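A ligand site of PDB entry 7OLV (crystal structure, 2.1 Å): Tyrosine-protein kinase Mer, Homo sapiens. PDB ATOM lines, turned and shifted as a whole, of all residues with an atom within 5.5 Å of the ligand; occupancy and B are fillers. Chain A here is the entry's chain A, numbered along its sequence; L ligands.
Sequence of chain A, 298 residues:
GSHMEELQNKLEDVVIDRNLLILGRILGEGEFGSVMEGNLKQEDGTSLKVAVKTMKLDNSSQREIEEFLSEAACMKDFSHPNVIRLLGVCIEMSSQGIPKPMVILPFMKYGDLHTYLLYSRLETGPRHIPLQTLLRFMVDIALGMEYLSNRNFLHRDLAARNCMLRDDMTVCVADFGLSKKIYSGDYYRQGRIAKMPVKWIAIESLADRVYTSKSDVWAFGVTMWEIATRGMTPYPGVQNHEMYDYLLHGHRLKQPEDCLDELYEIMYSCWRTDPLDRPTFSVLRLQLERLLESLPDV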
ATOM      1  N   LEU A  27     -15.332  23.487  11.991  1.00  0.00           N
ATOM      2  CA  LEU A  27     -16.449  23.250  11.062  1.00  0.00           C
ATOM      3  C   LEU A  27     -17.767  22.944  11.780  1.00  0.00           C
ATOM      4  O   LEU A  27     -18.826  22.999  11.169  1.00  0.00           O
ATOM      5  CB  LEU A  27     -16.123  22.068  10.154  1.00  0.00           C
ATOM      6  CG  LEU A  27     -14.776  22.138   9.444  1.00  0.00           C
ATOM      7  CD1 LEU A  27     -14.414  20.791   8.836  1.00  0.00           C
ATOM      8  CD2 LEU A  27     -14.800  23.242   8.389  1.00  0.00           C
ATOM      9  N   VAL A  35     -15.434  19.258  15.493  1.00  0.00           N
ATOM     10  CA  VAL A  35     -14.858  18.831  14.232  1.00  0.00           C
ATOM     11  C   VAL A  35     -14.134  20.026  13.642  1.00  0.00           C
ATOM     12  O   VAL A  35     -14.711  21.108  13.493  1.00  0.00           O
ATOM     13  CB  VAL A  35     -15.918  18.343  13.231  1.00  0.00           C
ATOM     14  CG1 VAL A  35     -15.254  17.860  11.940  1.00  0.00           C
ATOM     15  CG2 VAL A  35     -16.740  17.222  13.841  1.00  0.00           C
ATOM     16  N   ALA A  51     -10.194  15.798   8.211  1.00  0.00           N
ATOM     17  CA  ALA A  51     -11.080  16.263   9.275  1.00  0.00           C
ATOM     18  C   ALA A  51     -10.586  15.684  10.608  1.00  0.00           C
ATOM     19  O   ALA A  51     -10.137  14.543  10.665  1.00  0.00           O
ATOM     20  CB  ALA A  51     -12.521  15.854   9.024  1.00  0.00           C
ATOM     21  N   LYS A  53     -11.735  15.147  14.577  1.00  0.00           N
ATOM     22  CA  LYS A  53     -12.760  15.158  15.615  1.00  0.00           C
ATOM     23  C   LYS A  53     -12.120  15.097  16.996  1.00  0.00           C
ATOM     24  O   LYS A  53     -11.460  14.112  17.320  1.00  0.00           O
ATOM     25  CB  LYS A  53     -13.735  13.982  15.428  1.00  0.00           C
ATOM     26  CG  LYS A  53     -14.817  13.831  16.500  1.00  0.00           C
ATOM     27  CD  LYS A  53     -15.814  14.973  16.507  1.00  0.00           C
ATOM     28  CE  LYS A  53     -16.724  14.935  17.727  1.00  0.00           C
ATOM     29  NZ  LYS A  53     -17.789  13.899  17.592  1.00  0.00           N
ATOM     30  N   MET A  55     -12.744  14.823  21.016  1.00  0.00           N
ATOM     31  CA  MET A  55     -13.780  14.218  21.862  1.00  0.00           C
ATOM     32  C   MET A  55     -13.951  15.003  23.176  1.00  0.00           C
ATOM     33  O   MET A  55     -13.123  14.903  24.078  1.00  0.00           O
ATOM     34  CB  MET A  55     -13.451  12.739  22.168  1.00  0.00           C
ATOM     35  CG  MET A  55     -13.070  11.885  20.968  1.00  0.00           C
ATOM     36  SD  MET A  55     -14.322  11.773  19.668  1.00  0.00           S
ATOM     37  CE  MET A  55     -15.548  10.723  20.450  1.00  0.00           C
ATOM     38  N   GLU A  67      -8.786   2.555  26.519  1.00  0.00           N
ATOM     39  CA  GLU A  67     -10.005   2.029  25.914  1.00  0.00           C
ATOM     40  C   GLU A  67     -10.246   2.677  24.552  1.00  0.00           C
ATOM     41  O   GLU A  67     -10.593   2.009  23.574  1.00  0.00           O
ATOM     42  CB  GLU A  67     -11.197   2.327  26.833  1.00  0.00           C
ATOM     43  CG  GLU A  67     -12.532   1.768  26.400  1.00  0.00           C
ATOM     44  CD  GLU A  67     -13.604   1.900  27.470  1.00  0.00           C
ATOM     45  OE1 GLU A  67     -13.441   2.744  28.399  1.00  0.00           O
ATOM     46  OE2 GLU A  67     -14.605   1.161  27.400  1.00  0.00           O
ATOM     47  N   PHE A  68     -10.053   3.993  24.521  1.00  0.00           N
ATOM     48  CA  PHE A  68     -10.134   4.763  23.289  1.00  0.00           C
ATOM     49  C   PHE A  68      -9.093   4.304  22.253  1.00  0.00           C
ATOM     50  O   PHE A  68      -9.446   4.039  21.107  1.00  0.00           O
ATOM     51  CB  PHE A  68      -9.946   6.250  23.607  1.00  0.00           C
ATOM     52  CG  PHE A  68     -10.132   7.140  22.423  1.00  0.00           C
ATOM     53  CD1 PHE A  68     -11.395   7.558  22.052  1.00  0.00           C
ATOM     54  CD2 PHE A  68      -9.036   7.559  21.674  1.00  0.00           C
ATOM     55  CE1 PHE A  68     -11.576   8.389  20.958  1.00  0.00           C
ATOM     56  CE2 PHE A  68      -9.207   8.389  20.577  1.00  0.00           C
ATOM     57  CZ  PHE A  68     -10.478   8.799  20.219  1.00  0.00           C
ATOM     58  N   LEU A  69      -7.836   4.206  22.654  1.00  0.00           N
ATOM     59  CA  LEU A  69      -6.773   3.813  21.740  1.00  0.00           C
ATOM     60  C   LEU A  69      -6.974   2.400  21.219  1.00  0.00           C
ATOM     61  O   LEU A  69      -6.685   2.111  20.058  1.00  0.00           O
ATOM     62  CB  LEU A  69      -5.408   3.916  22.423  1.00  0.00           C
ATOM     63  CG  LEU A  69      -4.908   5.298  22.830  1.00  0.00           C
ATOM     64  CD1 LEU A  69      -3.603   5.126  23.602  1.00  0.00           C
ATOM     65  CD2 LEU A  69      -4.696   6.203  21.635  1.00  0.00           C
ATOM     66  N   GLU A  71      -9.883   0.755  20.962  1.00  0.00           N
ATOM     67  CA  GLU A  71     -11.024   0.851  20.067  1.00  0.00           C
ATOM     68  C   GLU A  71     -10.590   1.476  18.733  1.00  0.00           C
ATOM     69  O   GLU A  71     -10.869   0.930  17.669  1.00  0.00           O
ATOM     70  CB  GLU A  71     -12.125   1.674  20.756  1.00  0.00           C
ATOM     71  CG  GLU A  71     -13.456   1.762  20.012  1.00  0.00           C
ATOM     72  CD  GLU A  71     -14.300   0.502  20.120  1.00  0.00           C
ATOM     73  OE1 GLU A  71     -14.292  -0.139  21.202  1.00  0.00           O
ATOM     74  OE2 GLU A  71     -14.987   0.147  19.143  1.00  0.00           O
ATOM     75  N   ALA A  72      -9.880   2.583  18.795  1.00  0.00           N
ATOM     76  CA  ALA A  72      -9.328   3.245  17.601  1.00  0.00           C
ATOM     77  C   ALA A  72      -8.460   2.298  16.783  1.00  0.00           C
ATOM     78  O   ALA A  72      -8.555   2.287  15.555  1.00  0.00           O
ATOM     79  CB  ALA A  72      -8.540   4.481  17.992  1.00  0.00           C
ATOM     80  N   MET A  75     -10.660   0.101  14.632  1.00  0.00           N
ATOM     81  CA  MET A  75     -11.290   0.834  13.563  1.00  0.00           C
ATOM     82  C   MET A  75     -10.303   1.193  12.443  1.00  0.00           C
ATOM     83  O   MET A  75     -10.638   1.105  11.262  1.00  0.00           O
ATOM     84  CB  MET A  75     -11.941   2.114  14.104  1.00  0.00           C
ATOM     85  CG  MET A  75     -13.090   1.854  15.071  1.00  0.00           C
ATOM     86  SD  MET A  75     -13.579   3.363  15.928  1.00  0.00           S
ATOM     87  CE  MET A  75     -14.937   2.776  16.928  1.00  0.00           C
ATOM     88  N   ILE A  84     -15.589   4.355   6.375  1.00  0.00           N
ATOM     89  CA  ILE A  84     -14.655   5.477   6.444  1.00  0.00           C
ATOM     90  C   ILE A  84     -13.273   4.997   6.902  1.00  0.00           C
ATOM     91  O   ILE A  84     -13.179   4.182   7.822  1.00  0.00           O
ATOM     92  CB  ILE A  84     -15.176   6.602   7.362  1.00  0.00           C
ATOM     93  CG1 ILE A  84     -14.369   7.890   7.136  1.00  0.00           C
ATOM     94  CG2 ILE A  84     -15.162   6.189   8.837  1.00  0.00           C
ATOM     95  CD1 ILE A  84     -15.072   9.152   7.579  1.00  0.00           C
ATOM     96  N   LEU A  86     -10.210   5.395   8.884  1.00  0.00           N
ATOM     97  CA  LEU A  86      -9.578   6.110   9.995  1.00  0.00           C
ATOM     98  C   LEU A  86      -8.064   6.195   9.736  1.00  0.00           C
ATOM     99  O   LEU A  86      -7.402   5.163   9.594  1.00  0.00           O
ATOM    100  CB  LEU A  86      -9.840   5.392  11.320  1.00  0.00           C
ATOM    101  CG  LEU A  86      -9.136   5.907  12.578  1.00  0.00           C
ATOM    102  CD1 LEU A  86      -9.550   7.318  12.880  1.00  0.00           C
ATOM    103  CD2 LEU A  86      -9.432   5.011  13.766  1.00  0.00           C
ATOM    104  N   VAL A  89      -5.051   8.475  15.211  1.00  0.00           N
ATOM    105  CA  VAL A  89      -5.478   9.340  16.308  1.00  0.00           C
ATOM    106  C   VAL A  89      -4.283  10.079  16.898  1.00  0.00           C
ATOM    107  O   VAL A  89      -3.171   9.596  16.828  1.00  0.00           O
ATOM    108  CB  VAL A  89      -6.244   8.555  17.400  1.00  0.00           C
ATOM    109  CG1 VAL A  89      -7.441   7.825  16.799  1.00  0.00           C
ATOM    110  CG2 VAL A  89      -5.345   7.556  18.107  1.00  0.00           C
ATOM    111  N   VAL A 103      -9.404  12.377  16.496  1.00  0.00           N
ATOM    112  CA  VAL A 103      -9.603  11.367  15.449  1.00  0.00           C
ATOM    113  C   VAL A 103      -9.390  12.025  14.092  1.00  0.00           C
ATOM    114  O   VAL A 103     -10.068  12.990  13.754  1.00  0.00           O
ATOM    115  CB  VAL A 103     -11.034  10.799  15.516  1.00  0.00           C
ATOM    116  CG1 VAL A 103     -11.257   9.710  14.464  1.00  0.00           C
ATOM    117  CG2 VAL A 103     -11.322  10.224  16.897  1.00  0.00           C
ATOM    118  N   LEU A 105      -9.406  11.960  10.032  1.00  0.00           N
ATOM    119  CA  LEU A 105     -10.238  11.352   9.010  1.00  0.00           C
ATOM    120  C   LEU A 105      -9.974  12.027   7.677  1.00  0.00           C
ATOM    121  O   LEU A 105      -9.577  13.210   7.664  1.00  0.00           O
ATOM    122  CB  LEU A 105     -11.712  11.552   9.372  1.00  0.00           C
ATOM    123  CG  LEU A 105     -12.102  11.084  10.781  1.00  0.00           C
ATOM    124  CD1 LEU A 105     -13.481  11.567  11.137  1.00  0.00           C
ATOM    125  CD2 LEU A 105     -12.049   9.566  10.867  1.00  0.00           C
ATOM    126  N   PRO A 106     -10.200  11.325   6.552  1.00  0.00           N
ATOM    127  CA  PRO A 106     -10.131  12.009   5.265  1.00  0.00           C
ATOM    128  C   PRO A 106     -11.179  13.122   5.175  1.00  0.00           C
ATOM    129  O   PRO A 106     -12.311  12.930   5.628  1.00  0.00           O
ATOM    130  CB  PRO A 106     -10.443  10.903   4.240  1.00  0.00           C
ATOM    131  CG  PRO A 106     -10.383   9.620   4.990  1.00  0.00           C
ATOM    132  CD  PRO A 106     -10.657   9.945   6.416  1.00  0.00           C
ATOM    133  N   PHE A 107     -10.794  14.272   4.636  1.00  0.00           N
ATOM    134  CA  PHE A 107     -11.738  15.374   4.475  1.00  0.00           C
ATOM    135  C   PHE A 107     -12.730  15.064   3.351  1.00  0.00           C
ATOM    136  O   PHE A 107     -12.327  14.707   2.227  1.00  0.00           O
ATOM    137  CB  PHE A 107     -11.014  16.677   4.208  1.00  0.00           C
ATOM    138  CG  PHE A 107     -11.894  17.893   4.331  1.00  0.00           C
ATOM    139  CD1 PHE A 107     -12.118  18.479   5.566  1.00  0.00           C
ATOM    140  CD2 PHE A 107     -12.496  18.442   3.199  1.00  0.00           C
ATOM    141  CE1 PHE A 107     -12.925  19.593   5.669  1.00  0.00           C
ATOM    142  CE2 PHE A 107     -13.303  19.555   3.302  1.00  0.00           C
ATOM    143  CZ  PHE A 107     -13.518  20.130   4.536  1.00  0.00           C
ATOM    144  N   MET A 108     -14.014  15.207   3.675  1.00  0.00           N
ATOM    145  CA  MET A 108     -15.132  14.847   2.813  1.00  0.00           C
ATOM    146  C   MET A 108     -15.902  16.125   2.457  1.00  0.00           C
ATOM    147  O   MET A 108     -16.813  16.536   3.189  1.00  0.00           O
ATOM    148  CB  MET A 108     -16.056  13.891   3.571  1.00  0.00           C
ATOM    149  CG  MET A 108     -15.392  12.644   4.132  1.00  0.00           C
ATOM    150  SD  MET A 108     -15.701  11.195   3.122  1.00  0.00           S
ATOM    151  CE  MET A 108     -14.991   9.906   4.145  1.00  0.00           C
ATOM    152  N   LYS A 109     -15.533  16.758   1.340  1.00  0.00           N
ATOM    153  CA  LYS A 109     -16.109  18.075   0.987  1.00  0.00           C
ATOM    154  C   LYS A 109     -17.641  18.046   0.763  1.00  0.00           C
ATOM    155  O   LYS A 109     -18.314  19.031   1.007  1.00  0.00           O
ATOM    156  CB  LYS A 109     -15.366  18.703  -0.217  1.00  0.00           C
ATOM    157  CG  LYS A 109     -15.557  17.978  -1.548  1.00  0.00           C
ATOM    158  CD  LYS A 109     -14.862  18.690  -2.705  1.00  0.00           C
ATOM    159  CE  LYS A 109     -14.969  17.861  -3.977  1.00  0.00           C
ATOM    160  NZ  LYS A 109     -15.227  18.684  -5.195  1.00  0.00           N
ATOM    161  N   GLY A 111     -19.691  16.261   2.512  1.00  0.00           N
ATOM    162  CA  GLY A 111     -20.277  16.231   3.836  1.00  0.00           C
ATOM    163  C   GLY A 111     -21.070  14.967   4.097  1.00  0.00           C
ATOM    164  O   GLY A 111     -20.840  13.924   3.453  1.00  0.00           O
ATOM    165  N   MET A 164     -21.014   9.323   5.206  1.00  0.00           N
ATOM    166  CA  MET A 164     -20.336  10.431   4.534  1.00  0.00           C
ATOM    167  C   MET A 164     -20.231  10.156   3.037  1.00  0.00           C
ATOM    168  O   MET A 164     -20.226   9.019   2.615  1.00  0.00           O
ATOM    169  CB  MET A 164     -18.975  10.661   5.173  1.00  0.00           C
ATOM    170  CG  MET A 164     -19.010  10.988   6.665  1.00  0.00           C
ATOM    171  SD  MET A 164     -19.691  12.598   7.148  1.00  0.00           S
ATOM    172  CE  MET A 164     -18.640  13.733   6.250  1.00  0.00           C
ATOM    173  N   ALA A 174     -19.782   5.934   8.828  1.00  0.00           N
ATOM    174  CA  ALA A 174     -18.825   6.655   9.667  1.00  0.00           C
ATOM    175  C   ALA A 174     -19.424   6.929  11.045  1.00  0.00           C
ATOM    176  O   ALA A 174     -20.526   6.457  11.341  1.00  0.00           O
ATOM    177  CB  ALA A 174     -18.453   7.960   8.989  1.00  0.00           C
ATOM    178  N   ASP A 175     -18.693   7.675  11.883  1.00  0.00           N
ATOM    179  CA  ASP A 175     -19.187   8.179  13.175  1.00  0.00           C
ATOM    180  C   ASP A 175     -19.715   7.077  14.085  1.00  0.00           C
ATOM    181  O   ASP A 175     -20.822   7.145  14.597  1.00  0.00           O
ATOM    182  CB  ASP A 175     -20.257   9.288  12.966  1.00  0.00           C
ATOM    183  CG  ASP A 175     -19.721  10.687  13.225  1.00  0.00           C
ATOM    184  OD1 ASP A 175     -18.995  10.856  14.221  1.00  0.00           O
ATOM    185  OD2 ASP A 175     -20.061  11.613  12.458  1.00  0.00           O
ATOM    186  N   PHE A 176     -18.883   6.070  14.320  1.00  0.00           N
ATOM    187  CA  PHE A 176     -19.318   4.881  15.046  1.00  0.00           C
ATOM    188  C   PHE A 176     -19.689   5.211  16.499  1.00  0.00           C
ATOM    189  O   PHE A 176     -19.023   6.028  17.139  1.00  0.00           O
ATOM    190  CB  PHE A 176     -18.244   3.803  14.978  1.00  0.00           C
ATOM    191  CG  PHE A 176     -17.754   3.520  13.590  1.00  0.00           C
ATOM    192  CD1 PHE A 176     -18.624   3.018  12.641  1.00  0.00           C
ATOM    193  CD2 PHE A 176     -16.434   3.783  13.212  1.00  0.00           C
ATOM    194  CE1 PHE A 176     -18.203   2.754  11.334  1.00  0.00           C
ATOM    195  CE2 PHE A 176     -16.000   3.528  11.910  1.00  0.00           C
ATOM    196  CZ  PHE A 176     -16.879   3.009  10.975  1.00  0.00           C
ATOM    197  N   GLY A 177     -20.770   4.591  16.994  1.00  0.00           N
ATOM    198  CA  GLY A 177     -21.285   4.861  18.338  1.00  0.00           C
ATOM    199  C   GLY A 177     -20.410   4.297  19.444  1.00  0.00           C
ATOM    200  O   GLY A 177     -20.210   4.948  20.466  1.00  0.00           O
HETATM  201  C1  LIG L   1     -17.763  13.101  10.251  1.00  0.00           C
HETATM  202  C2  LIG L   1     -16.935  13.760   9.187  1.00  0.00           C
HETATM  203  C3  LIG L   1     -15.846  13.042   8.511  1.00  0.00           C
HETATM  204  N1  LIG L   1     -13.081   5.827  18.949  1.00  0.00           N
HETATM  205  C4  LIG L   1     -16.408  16.949   7.370  1.00  0.00           C
HETATM  206  C5  LIG L   1     -17.144  15.057   8.845  1.00  0.00           C
HETATM  207  C6  LIG L   1     -16.713  11.446  11.687  1.00  0.00           C
HETATM  208  C7  LIG L   1     -15.981   9.792  12.806  1.00  0.00           C
HETATM  209  C8  LIG L   1     -15.465   9.053  13.961  1.00  0.00           C
HETATM  210  C9  LIG L   1     -15.552   9.668  15.218  1.00  0.00           C
HETATM  211  C10 LIG L   1     -15.112   9.016  16.354  1.00  0.00           C
HETATM  212  C11 LIG L   1     -14.591   7.733  16.259  1.00  0.00           C
HETATM  213  C12 LIG L   1     -14.541   7.106  15.025  1.00  0.00           C
HETATM  214  C13 LIG L   1     -14.971   7.742  13.856  1.00  0.00           C
HETATM  215  C14 LIG L   1     -14.999   6.676  18.585  1.00  0.00           C
HETATM  216  C15 LIG L   1     -16.424   7.039  18.842  1.00  0.00           C
HETATM  217  C16 LIG L   1     -12.068   5.086  19.700  1.00  0.00           C
HETATM  218  C17 LIG L   1     -12.965   6.424  17.731  1.00  0.00           C
HETATM  219  N2  LIG L   1     -10.767   6.362  16.412  1.00  0.00           N
HETATM  220  C18 LIG L   1     -11.757   6.404  16.987  1.00  0.00           C
HETATM  221  N3  LIG L   1     -14.317   5.983  19.478  1.00  0.00           N
HETATM  222  C19 LIG L   1     -14.163   7.002  17.471  1.00  0.00           C
HETATM  223  C20 LIG L   1     -14.863   6.996  12.556  1.00  0.00           C
HETATM  224  O1  LIG L   1     -16.206  11.145  12.912  1.00  0.00           O
HETATM  225  N4  LIG L   1     -16.354   9.308  11.668  1.00  0.00           N
HETATM  226  N5  LIG L   1     -16.824  10.393  10.912  1.00  0.00           N
HETATM  227  N6  LIG L   1     -17.023  12.718  11.450  1.00  0.00           N
HETATM  228  C21 LIG L   1     -16.604  13.803  12.341  1.00  0.00           C
HETATM  229  N7  LIG L   1     -16.372  15.665   7.876  1.00  0.00           N
HETATM  230  C22 LIG L   1     -15.435  17.012   6.444  1.00  0.00           C
HETATM  231  N8  LIG L   1     -14.760  15.810   6.327  1.00  0.00           N
HETATM  232  C23 LIG L   1     -15.336  14.994   7.209  1.00  0.00           C
HETATM  233  C24 LIG L   1     -15.082  13.642   7.555  1.00  0.00           C
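A nitrogen (N8) of the ligand lies within hydrogen-bond range of the backbone NH of Met 108, at 2.8 Å. The backbone NH of Asp 175 sits at hydrogen-bond distance from a nitrogen (N4) of the ligand, at 2.9 Å.
O of Leu 105 is in hydrogen-bond range of N of Ala 51 (2.7 Å). N of Leu 27 lies within hydrogen-bond range of O of Val 35, 2.9 Å away. N of Val 103 lies within hydrogen-bond range of O of Lys 53 (2.8 Å).
Residues that only touch the ligand: Phe 68 (3.2 Å), Leu 86 (3.3 Å), Phe 176 (3.3 Å), Met 164 (3.3 Å), Leu 105 (3.3 Å), Ala 72 (3.3 Å), Pro 106 (3.4 Å), Ala 51 (3.5 Å), Ala 174 (3.5 Å), Phe 107 (3.6 Å), Glu 71 (3.6 Å), Met 75 (3.6 Å), Val 89 (3.7 Å), Val 35 (3.7 Å), Ile 84 (3.8 Å) and Val 103 (3.8 Å). Hydrophobic or aromatic side chains that line the ligand: Val 35, Ala 51, Phe 68, Ala 72, Met 75, Ile 84, Leu 86, Val 89, Val 103, Leu 105, Phe 107, Met 108, Met 164, Ala 174 and Phe 176. Of the 26 residues printed, 18 come within 4 Å of the ligand. The nearest printed residue that does not touch the ligand is Met 55 (4.1 Å).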
